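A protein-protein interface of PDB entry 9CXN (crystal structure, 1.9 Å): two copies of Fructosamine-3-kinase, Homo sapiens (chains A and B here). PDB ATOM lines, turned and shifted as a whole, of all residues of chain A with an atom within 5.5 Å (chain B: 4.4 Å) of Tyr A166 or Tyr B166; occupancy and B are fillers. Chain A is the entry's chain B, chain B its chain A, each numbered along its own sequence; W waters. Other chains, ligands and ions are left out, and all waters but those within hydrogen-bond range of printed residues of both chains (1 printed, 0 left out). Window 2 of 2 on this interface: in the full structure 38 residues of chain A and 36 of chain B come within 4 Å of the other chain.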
ATOM      1  N   LEU A 161      24.558  17.638 -21.106  1.00  0.00           N
ATOM      2  CA  LEU A 161      24.884  16.272 -20.722  1.00  0.00           C
ATOM      3  C   LEU A 161      23.986  15.765 -19.584  1.00  0.00           C
ATOM      4  O   LEU A 161      23.548  14.605 -19.611  1.00  0.00           O
ATOM      5  CB  LEU A 161      26.389  16.198 -20.349  1.00  0.00           C
ATOM      6  CG  LEU A 161      26.968  14.822 -20.110  1.00  0.00           C
ATOM      7  CD1 LEU A 161      26.623  13.823 -21.254  1.00  0.00           C
ATOM      8  CD2 LEU A 161      28.558  14.981 -19.926  1.00  0.00           C
ATOM      9  N   ILE A 162      23.709  16.602 -18.566  1.00  0.00           N
ATOM     10  CA  ILE A 162      22.776  16.198 -17.521  1.00  0.00           C
ATOM     11  C   ILE A 162      21.410  15.881 -18.132  1.00  0.00           C
ATOM     12  O   ILE A 162      20.738  14.902 -17.745  1.00  0.00           O
ATOM     13  CB  ILE A 162      22.692  17.305 -16.459  1.00  0.00           C
ATOM     14  CG1 ILE A 162      23.962  17.202 -15.566  1.00  0.00           C
ATOM     15  CG2 ILE A 162      21.421  17.229 -15.558  1.00  0.00           C
ATOM     16  CD1 ILE A 162      24.257  18.552 -14.926  1.00  0.00           C
ATOM     17  N   GLU A 163      20.969  16.709 -19.085  1.00  0.00           N
ATOM     18  CA  GLU A 163      19.660  16.472 -19.724  1.00  0.00           C
ATOM     19  C   GLU A 163      19.667  15.167 -20.503  1.00  0.00           C
ATOM     20  O   GLU A 163      18.710  14.368 -20.432  1.00  0.00           O
ATOM     21  CB  GLU A 163      19.314  17.642 -20.653  1.00  0.00           C
ATOM     22  CG  GLU A 163      18.016  17.390 -21.446  1.00  0.00           C
ATOM     23  CD  GLU A 163      16.759  17.213 -20.579  1.00  0.00           C
ATOM     24  OE1 GLU A 163      16.649  17.530 -19.373  1.00  0.00           O
ATOM     25  OE2 GLU A 163      15.789  16.769 -21.146  1.00  0.00           O
ATOM     26  N   LYS A 164      20.715  14.935 -21.270  1.00  0.00           N
ATOM     27  CA  LYS A 164      20.819  13.676 -22.006  1.00  0.00           C
ATOM     28  C   LYS A 164      20.786  12.477 -21.054  1.00  0.00           C
ATOM     29  O   LYS A 164      20.051  11.502 -21.272  1.00  0.00           O
ATOM     30  CB  LYS A 164      22.099  13.676 -22.822  1.00  0.00           C
ATOM     31  CG  LYS A 164      22.425  12.451 -23.701  1.00  0.00           C
ATOM     32  CD  LYS A 164      23.949  12.460 -24.095  1.00  0.00           C
ATOM     33  CE  LYS A 164      24.137  12.196 -25.573  1.00  0.00           C
ATOM     34  NZ  LYS A 164      23.995  10.738 -25.893  1.00  0.00           N
ATOM     35  N   ASP A 165      21.580  12.517 -20.004  1.00  0.00           N
ATOM     36  CA  ASP A 165      21.800  11.292 -19.219  1.00  0.00           C
ATOM     37  C   ASP A 165      20.853  11.124 -18.039  1.00  0.00           C
ATOM     38  O   ASP A 165      20.525   9.976 -17.660  1.00  0.00           O
ATOM     39  CB  ASP A 165      23.264  11.274 -18.718  1.00  0.00           C
ATOM     40  CG  ASP A 165      24.260  11.035 -19.838  1.00  0.00           C
ATOM     41  OD1 ASP A 165      23.848  10.632 -20.945  1.00  0.00           O
ATOM     42  OD2 ASP A 165      25.476  11.252 -19.626  1.00  0.00           O
ATOM     43  N   TYR A 166      20.382  12.225 -17.451  1.00  0.00           N
ATOM     44  CA  TYR A 166      19.496  12.191 -16.305  1.00  0.00           C
ATOM     45  C   TYR A 166      18.118  12.741 -16.616  1.00  0.00           C
ATOM     46  O   TYR A 166      17.188  12.523 -15.827  1.00  0.00           O
ATOM     47  CB  TYR A 166      20.071  12.968 -15.101  1.00  0.00           C
ATOM     48  CG  TYR A 166      21.420  12.457 -14.651  1.00  0.00           C
ATOM     49  CD1 TYR A 166      21.538  11.347 -13.786  1.00  0.00           C
ATOM     50  CD2 TYR A 166      22.581  13.037 -15.093  1.00  0.00           C
ATOM     51  CE1 TYR A 166      22.802  10.852 -13.383  1.00  0.00           C
ATOM     52  CE2 TYR A 166      23.838  12.560 -14.680  1.00  0.00           C
ATOM     53  CZ  TYR A 166      23.957  11.447 -13.836  1.00  0.00           C
ATOM     54  OH  TYR A 166      25.264  11.028 -13.491  1.00  0.00           O
ATOM     55  N   ALA A 167      17.961  13.459 -17.713  1.00  0.00           N
ATOM     56  CA  ALA A 167      16.656  14.091 -18.078  1.00  0.00           C
ATOM     57  C   ALA A 167      15.992  14.770 -16.870  1.00  0.00           C
ATOM     58  O   ALA A 167      14.805  14.588 -16.566  1.00  0.00           O
ATOM     59  CB  ALA A 167      15.718  13.056 -18.741  1.00  0.00           C
ATOM     60  N   ASP A 168      16.780  15.592 -16.158  1.00  0.00           N
ATOM     61  CA  ASP A 168      16.356  16.158 -14.875  1.00  0.00           C
ATOM     62  C   ASP A 168      15.571  17.460 -15.072  1.00  0.00           C
ATOM     63  O   ASP A 168      16.140  18.483 -15.489  1.00  0.00           O
ATOM     64  CB  ASP A 168      17.578  16.382 -13.986  1.00  0.00           C
ATOM     65  CG  ASP A 168      17.201  16.659 -12.569  1.00  0.00           C
ATOM     66  OD1 ASP A 168      16.764  17.792 -12.279  1.00  0.00           O
ATOM     67  OD2 ASP A 168      17.372  15.783 -11.712  1.00  0.00           O
ATOM     68  N   TRP A 271      28.533  15.905 -10.976  1.00  0.00           N
ATOM     69  CA  TRP A 271      27.303  15.178 -11.279  1.00  0.00           C
ATOM     70  C   TRP A 271      27.471  14.342 -12.523  1.00  0.00           C
ATOM     71  O   TRP A 271      27.097  13.130 -12.525  1.00  0.00           O
ATOM     72  CB  TRP A 271      26.130  16.125 -11.414  1.00  0.00           C
ATOM     73  CG  TRP A 271      24.713  15.477 -11.520  1.00  0.00           C
ATOM     74  CD1 TRP A 271      24.360  14.133 -11.585  1.00  0.00           C
ATOM     75  CD2 TRP A 271      23.520  16.229 -11.633  1.00  0.00           C
ATOM     76  NE1 TRP A 271      22.947  14.029 -11.684  1.00  0.00           N
ATOM     77  CE2 TRP A 271      22.427  15.314 -11.702  1.00  0.00           C
ATOM     78  CE3 TRP A 271      23.261  17.621 -11.648  1.00  0.00           C
ATOM     79  CZ2 TRP A 271      21.079  15.748 -11.835  1.00  0.00           C
ATOM     80  CZ3 TRP A 271      21.929  18.051 -11.737  1.00  0.00           C
ATOM     81  CH2 TRP A 271      20.836  17.121 -11.840  1.00  0.00           C
ATOM     82  N   ASN A 272      28.083  14.903 -13.558  1.00  0.00           N
ATOM     83  CA  ASN A 272      28.263  14.126 -14.768  1.00  0.00           C
ATOM     84  C   ASN A 272      29.293  13.022 -14.591  1.00  0.00           C
ATOM     85  O   ASN A 272      29.093  11.910 -15.090  1.00  0.00           O
ATOM     86  CB  ASN A 272      28.652  14.997 -15.956  1.00  0.00           C
ATOM     87  CG  ASN A 272      27.407  15.657 -16.596  1.00  0.00           C
ATOM     88  OD1 ASN A 272      26.374  14.960 -16.820  1.00  0.00           O
ATOM     89  ND2 ASN A 272      27.477  16.976 -16.843  1.00  0.00           N
ATOM     90  N   PHE A 274      30.411  11.601 -11.626  1.00  0.00           N
ATOM     91  CA  PHE A 274      30.319  10.758 -10.455  1.00  0.00           C
ATOM     92  C   PHE A 274      28.897  10.511 -10.026  1.00  0.00           C
ATOM     93  O   PHE A 274      28.693   9.806  -9.029  1.00  0.00           O
ATOM     94  CB  PHE A 274      31.087  11.345  -9.269  1.00  0.00           C
ATOM     95  CG  PHE A 274      32.531  11.658  -9.581  1.00  0.00           C
ATOM     96  CD1 PHE A 274      33.393  10.665 -10.046  1.00  0.00           C
ATOM     97  CD2 PHE A 274      33.040  12.953  -9.421  1.00  0.00           C
ATOM     98  CE1 PHE A 274      34.736  10.950 -10.389  1.00  0.00           C
ATOM     99  CE2 PHE A 274      34.408  13.254  -9.746  1.00  0.00           C
ATOM    100  CZ  PHE A 274      35.251  12.263 -10.225  1.00  0.00           C
ATOM    101  N   GLY A 275      27.919  11.054 -10.727  1.00  0.00           N
ATOM    102  CA  GLY A 275      26.533  10.633 -10.519  1.00  0.00           C
ATOM    103  C   GLY A 275      25.721  11.454  -9.544  1.00  0.00           C
ATOM    104  O   GLY A 275      26.108  12.533  -9.078  1.00  0.00           O
ATOM    105  N   ARG A 276      24.597  10.874  -9.142  1.00  0.00           N
ATOM    106  CA  ARG A 276      23.508  11.617  -8.500  1.00  0.00           C
ATOM    107  C   ARG A 276      23.828  12.174  -7.125  1.00  0.00           C
ATOM    108  O   ARG A 276      23.095  13.052  -6.658  1.00  0.00           O
ATOM    109  CB  ARG A 276      22.247  10.728  -8.297  1.00  0.00           C
ATOM    110  CG  ARG A 276      21.629  10.323  -9.566  1.00  0.00           C
ATOM    111  N   ILE B 162      13.497   4.377 -10.812  1.00  0.00           N
ATOM    112  CA  ILE B 162      13.564   4.617 -12.243  1.00  0.00           C
ATOM    113  C   ILE B 162      12.228   5.147 -12.765  1.00  0.00           C
ATOM    114  O   ILE B 162      12.200   6.038 -13.629  1.00  0.00           O
ATOM    115  CB  ILE B 162      14.017   3.357 -12.997  1.00  0.00           C
ATOM    116  CG1 ILE B 162      15.562   3.230 -12.919  1.00  0.00           C
ATOM    117  CG2 ILE B 162      13.649   3.495 -14.440  1.00  0.00           C
ATOM    118  CD1 ILE B 162      16.087   1.798 -12.984  1.00  0.00           C
ATOM    119  N   GLU B 163      11.101   4.616 -12.257  1.00  0.00           N
ATOM    120  CA  GLU B 163       9.803   5.134 -12.696  1.00  0.00           C
ATOM    121  C   GLU B 163       9.619   6.594 -12.263  1.00  0.00           C
ATOM    122  O   GLU B 163       9.198   7.449 -13.057  1.00  0.00           O
ATOM    123  CB  GLU B 163       8.683   4.253 -12.140  1.00  0.00           C
ATOM    124  CG  GLU B 163       7.280   4.777 -12.401  1.00  0.00           C
ATOM    125  CD  GLU B 163       6.864   4.860 -13.878  1.00  0.00           C
ATOM    126  OE1 GLU B 163       5.729   5.307 -14.107  1.00  0.00           O
ATOM    127  OE2 GLU B 163       7.612   4.493 -14.804  1.00  0.00           O
ATOM    128  N   LYS B 164       9.938   6.888 -11.006  1.00  0.00           N
ATOM    129  CA  LYS B 164       9.823   8.240 -10.480  1.00  0.00           C
ATOM    130  C   LYS B 164      10.633   9.230 -11.303  1.00  0.00           C
ATOM    131  O   LYS B 164      10.109  10.271 -11.721  1.00  0.00           O
ATOM    132  CB  LYS B 164      10.267   8.257  -9.024  1.00  0.00           C
ATOM    133  CG  LYS B 164      10.103   9.612  -8.373  1.00  0.00           C
ATOM    134  CD  LYS B 164       9.834   9.495  -6.887  1.00  0.00           C
ATOM    135  CE  LYS B 164      11.077   9.748  -6.042  1.00  0.00           C
ATOM    136  NZ  LYS B 164      11.581  11.142  -6.223  1.00  0.00           N
ATOM    137  N   ASP B 165      11.908   8.916 -11.570  1.00  0.00           N
ATOM    138  CA  ASP B 165      12.805   9.883 -12.172  1.00  0.00           C
ATOM    139  C   ASP B 165      12.831   9.842 -13.680  1.00  0.00           C
ATOM    140  O   ASP B 165      13.262  10.810 -14.294  1.00  0.00           O
ATOM    141  CB  ASP B 165      14.258   9.700 -11.709  1.00  0.00           C
ATOM    142  CG  ASP B 165      14.458  10.000 -10.251  1.00  0.00           C
ATOM    143  OD1 ASP B 165      13.578  10.659  -9.637  1.00  0.00           O
ATOM    144  OD2 ASP B 165      15.505   9.579  -9.707  1.00  0.00           O
ATOM    145  N   TYR B 166      12.525   8.719 -14.309  1.00  0.00           N
ATOM    146  CA  TYR B 166      12.634   8.615 -15.746  1.00  0.00           C
ATOM    147  C   TYR B 166      11.340   8.285 -16.432  1.00  0.00           C
ATOM    148  O   TYR B 166      11.274   8.461 -17.647  1.00  0.00           O
ATOM    149  CB  TYR B 166      13.681   7.558 -16.157  1.00  0.00           C
ATOM    150  CG  TYR B 166      15.075   7.884 -15.727  1.00  0.00           C
ATOM    151  CD1 TYR B 166      15.536   7.507 -14.471  1.00  0.00           C
ATOM    152  CD2 TYR B 166      15.945   8.567 -16.580  1.00  0.00           C
ATOM    153  CE1 TYR B 166      16.822   7.801 -14.053  1.00  0.00           C
ATOM    154  CE2 TYR B 166      17.246   8.872 -16.172  1.00  0.00           C
ATOM    155  CZ  TYR B 166      17.662   8.506 -14.915  1.00  0.00           C
ATOM    156  OH  TYR B 166      18.931   8.788 -14.504  1.00  0.00           O
ATOM    157  N   ALA B 167      10.319   7.791 -15.697  1.00  0.00           N
ATOM    158  CA  ALA B 167       9.044   7.331 -16.272  1.00  0.00           C
ATOM    159  C   ALA B 167       9.282   6.465 -17.500  1.00  0.00           C
ATOM    160  O   ALA B 167       8.697   6.661 -18.570  1.00  0.00           O
ATOM    161  CB  ALA B 167       8.105   8.497 -16.593  1.00  0.00           C
ATOM    162  N   ASP B 168      10.147   5.464 -17.338  1.00  0.00           N
ATOM    163  CA  ASP B 168      10.562   4.663 -18.479  1.00  0.00           C
ATOM    164  C   ASP B 168       9.535   3.557 -18.764  1.00  0.00           C
ATOM    165  O   ASP B 168       9.346   2.641 -17.947  1.00  0.00           O
ATOM    166  CB  ASP B 168      11.947   4.076 -18.246  1.00  0.00           C
ATOM    167  CG  ASP B 168      12.547   3.558 -19.507  1.00  0.00           C
ATOM    168  OD1 ASP B 168      12.259   2.395 -19.855  1.00  0.00           O
ATOM    169  OD2 ASP B 168      13.288   4.302 -20.166  1.00  0.00           O
ATOM    170  N   TRP B 271      22.079   2.699 -13.363  1.00  0.00           N
ATOM    171  CA  TRP B 271      21.173   3.645 -14.009  1.00  0.00           C
ATOM    172  C   TRP B 271      20.708   4.727 -13.035  1.00  0.00           C
ATOM    173  O   TRP B 271      20.776   5.928 -13.373  1.00  0.00           O
ATOM    174  CB  TRP B 271      19.987   2.880 -14.613  1.00  0.00           C
ATOM    175  CG  TRP B 271      18.953   3.660 -15.465  1.00  0.00           C
ATOM    176  CD1 TRP B 271      18.869   5.036 -15.668  1.00  0.00           C
ATOM    177  CD2 TRP B 271      17.849   3.087 -16.171  1.00  0.00           C
ATOM    178  NE1 TRP B 271      17.785   5.322 -16.488  1.00  0.00           N
ATOM    179  CE2 TRP B 271      17.150   4.152 -16.811  1.00  0.00           C
ATOM    180  CE3 TRP B 271      17.382   1.759 -16.350  1.00  0.00           C
ATOM    181  CZ2 TRP B 271      15.984   3.930 -17.567  1.00  0.00           C
ATOM    182  CZ3 TRP B 271      16.249   1.540 -17.120  1.00  0.00           C
ATOM    183  CH2 TRP B 271      15.555   2.617 -17.721  1.00  0.00           C
ATOM    184  N   HIS B 273      22.277   5.688 -10.347  1.00  0.00           N
ATOM    185  CA  HIS B 273      23.423   6.501  -9.936  1.00  0.00           C
ATOM    186  C   HIS B 273      23.959   7.410 -11.051  1.00  0.00           C
ATOM    187  O   HIS B 273      24.317   8.572 -10.798  1.00  0.00           O
ATOM    188  CB  HIS B 273      24.554   5.625  -9.424  1.00  0.00           C
ATOM    189  CG  HIS B 273      24.407   5.267  -7.982  1.00  0.00           C
ATOM    190  ND1 HIS B 273      23.593   4.228  -7.545  1.00  0.00           N
ATOM    191  CD2 HIS B 273      24.881   5.870  -6.861  1.00  0.00           C
ATOM    192  CE1 HIS B 273      23.651   4.160  -6.223  1.00  0.00           C
ATOM    193  NE2 HIS B 273      24.401   5.163  -5.780  1.00  0.00           N
ATOM    194  N   PHE B 274      24.055   6.902 -12.266  1.00  0.00           N
ATOM    195  CA  PHE B 274      24.841   7.489 -13.339  1.00  0.00           C
ATOM    196  C   PHE B 274      24.030   7.781 -14.595  1.00  0.00           C
ATOM    197  O   PHE B 274      24.602   8.239 -15.588  1.00  0.00           O
ATOM    198  CB  PHE B 274      26.031   6.557 -13.664  1.00  0.00           C
ATOM    199  CG  PHE B 274      26.807   6.135 -12.466  1.00  0.00           C
ATOM    200  CD1 PHE B 274      27.497   7.079 -11.685  1.00  0.00           C
ATOM    201  CD2 PHE B 274      26.926   4.794 -12.110  1.00  0.00           C
ATOM    202  CE1 PHE B 274      28.201   6.706 -10.551  1.00  0.00           C
ATOM    203  CE2 PHE B 274      27.661   4.415 -11.006  1.00  0.00           C
ATOM    204  CZ  PHE B 274      28.304   5.361 -10.224  1.00  0.00           C
ATOM    205  N   GLY B 275      22.740   7.491 -14.614  1.00  0.00           N
ATOM    206  CA  GLY B 275      21.894   7.873 -15.734  1.00  0.00           C
ATOM    207  C   GLY B 275      21.785   6.839 -16.855  1.00  0.00           C
ATOM    208  O   GLY B 275      22.084   5.636 -16.719  1.00  0.00           O
ATOM    209  N   ARG B 276      21.354   7.340 -18.010  1.00  0.00           N
ATOM    210  CA  ARG B 276      20.848   6.489 -19.082  1.00  0.00           C
ATOM    211  C   ARG B 276      21.919   5.678 -19.802  1.00  0.00           C
ATOM    212  O   ARG B 276      21.551   4.825 -20.611  1.00  0.00           O
ATOM    213  CB  ARG B 276      20.017   7.321 -20.061  1.00  0.00           C
ATOM    214  CG  ARG B 276      18.706   7.807 -19.440  1.00  0.00           C
ATOM    215  CD  ARG B 276      17.885   8.713 -20.408  1.00  0.00           C
ATOM    216  NE  ARG B 276      16.913   7.935 -21.174  1.00  0.00           N
ATOM    217  CZ  ARG B 276      17.093   7.511 -22.423  1.00  0.00           C
ATOM    218  NH1 ARG B 276      18.196   7.786 -23.101  1.00  0.00           N
ATOM    219  NH2 ARG B 276      16.149   6.768 -22.999  1.00  0.00           N
HETATM  220  O   HOH W   1      26.901  10.039 -15.608  1.00  0.00           O
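Of the 12 printed residues of chain B, 5 touch a printed residue of chain A.
Hydrophobic or aromatic side chains of chain B that line the printed part of chain A: Tyr B166 and Phe B274.
Along chain B the printed residues that touch a printed residue of chain A span positions 166 to 276.
Among the printed residues, 12 pairs touch across the chains.
Among the printed residues, no Asp or Glu carboxylate lies within 4 Å of a Lys or Arg side-chain nitrogen of the other chain.
Among the printed residues, pairs that only touch across the chains: Lys A164 with Arg B276, Asp A165 with Tyr B166, Asp A165 with Gly B275, Tyr A166 with Tyr B166, Tyr A166 with His B273, Tyr A166 with Phe B274, Tyr A166 with Gly B275, Phe A274 with Phe B274, Gly A275 with His B273 and Gly A275 with Phe B274.
Water W1 lies within hydrogen-bond range of the side-chain hydroxyl of Tyr A166 (2.9 Å), the backbone carbonyl oxygen of Phe B274 (2.9 Å) and the backbone carbonyl oxygen of Asn A272 (2.9 Å).
Of the printed residues of chain B, Tyr A166 touches Tyr B166 (3.7 Å), His B273 (3.8 Å), Phe B274 (3.5 Å) and Gly B275 (3.6 Å).
Of the printed residues of chain B, Gly A275 touches His B273 and Phe B274.
Printed residues of chain B within 4 Å of Arg A276: His B273 (2.8 Å).
Printed residues of chain A within 4 Å of Tyr B166: Asp A165 (3.7 Å) and Tyr A166 (3.7 Å).
Of the printed residues of chain A, Phe B274 touches Tyr A166, Phe A274 and Gly A275.
Of the printed residues of chain A, Gly B275 touches Asp A165 and Tyr A166.
The nearest printed residue of chain B that does not touch Tyr A166 is Asp B165 (4.5 Å).
The nearest printed residue of chain A that does not touch His B273 is Phe A274 (4.9 Å).
O of Trp A271 sits at hydrogen-bond distance from OH of Tyr A166 (3.0 Å).
Lys A164 touches Arg B276, but with the chains exchanged Arg A276 does not touch Lys B164 (10.6 Å).
Tyr B166 touches its own counterpart, Tyr A166.
Tyr A166 touches Phe B274, but with the chains exchanged Phe A274 does not touch Tyr B166 (11.1 Å).
Phe A274 touches its own counterpart, Phe B274.
O of His B273 is in hydrogen-bond range of N of Arg A276 (2.8 Å).
The backbone NH of Arg B276 sits at hydrogen-bond distance from the backbone carbonyl oxygen of Asp A165 (2.8 Å).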
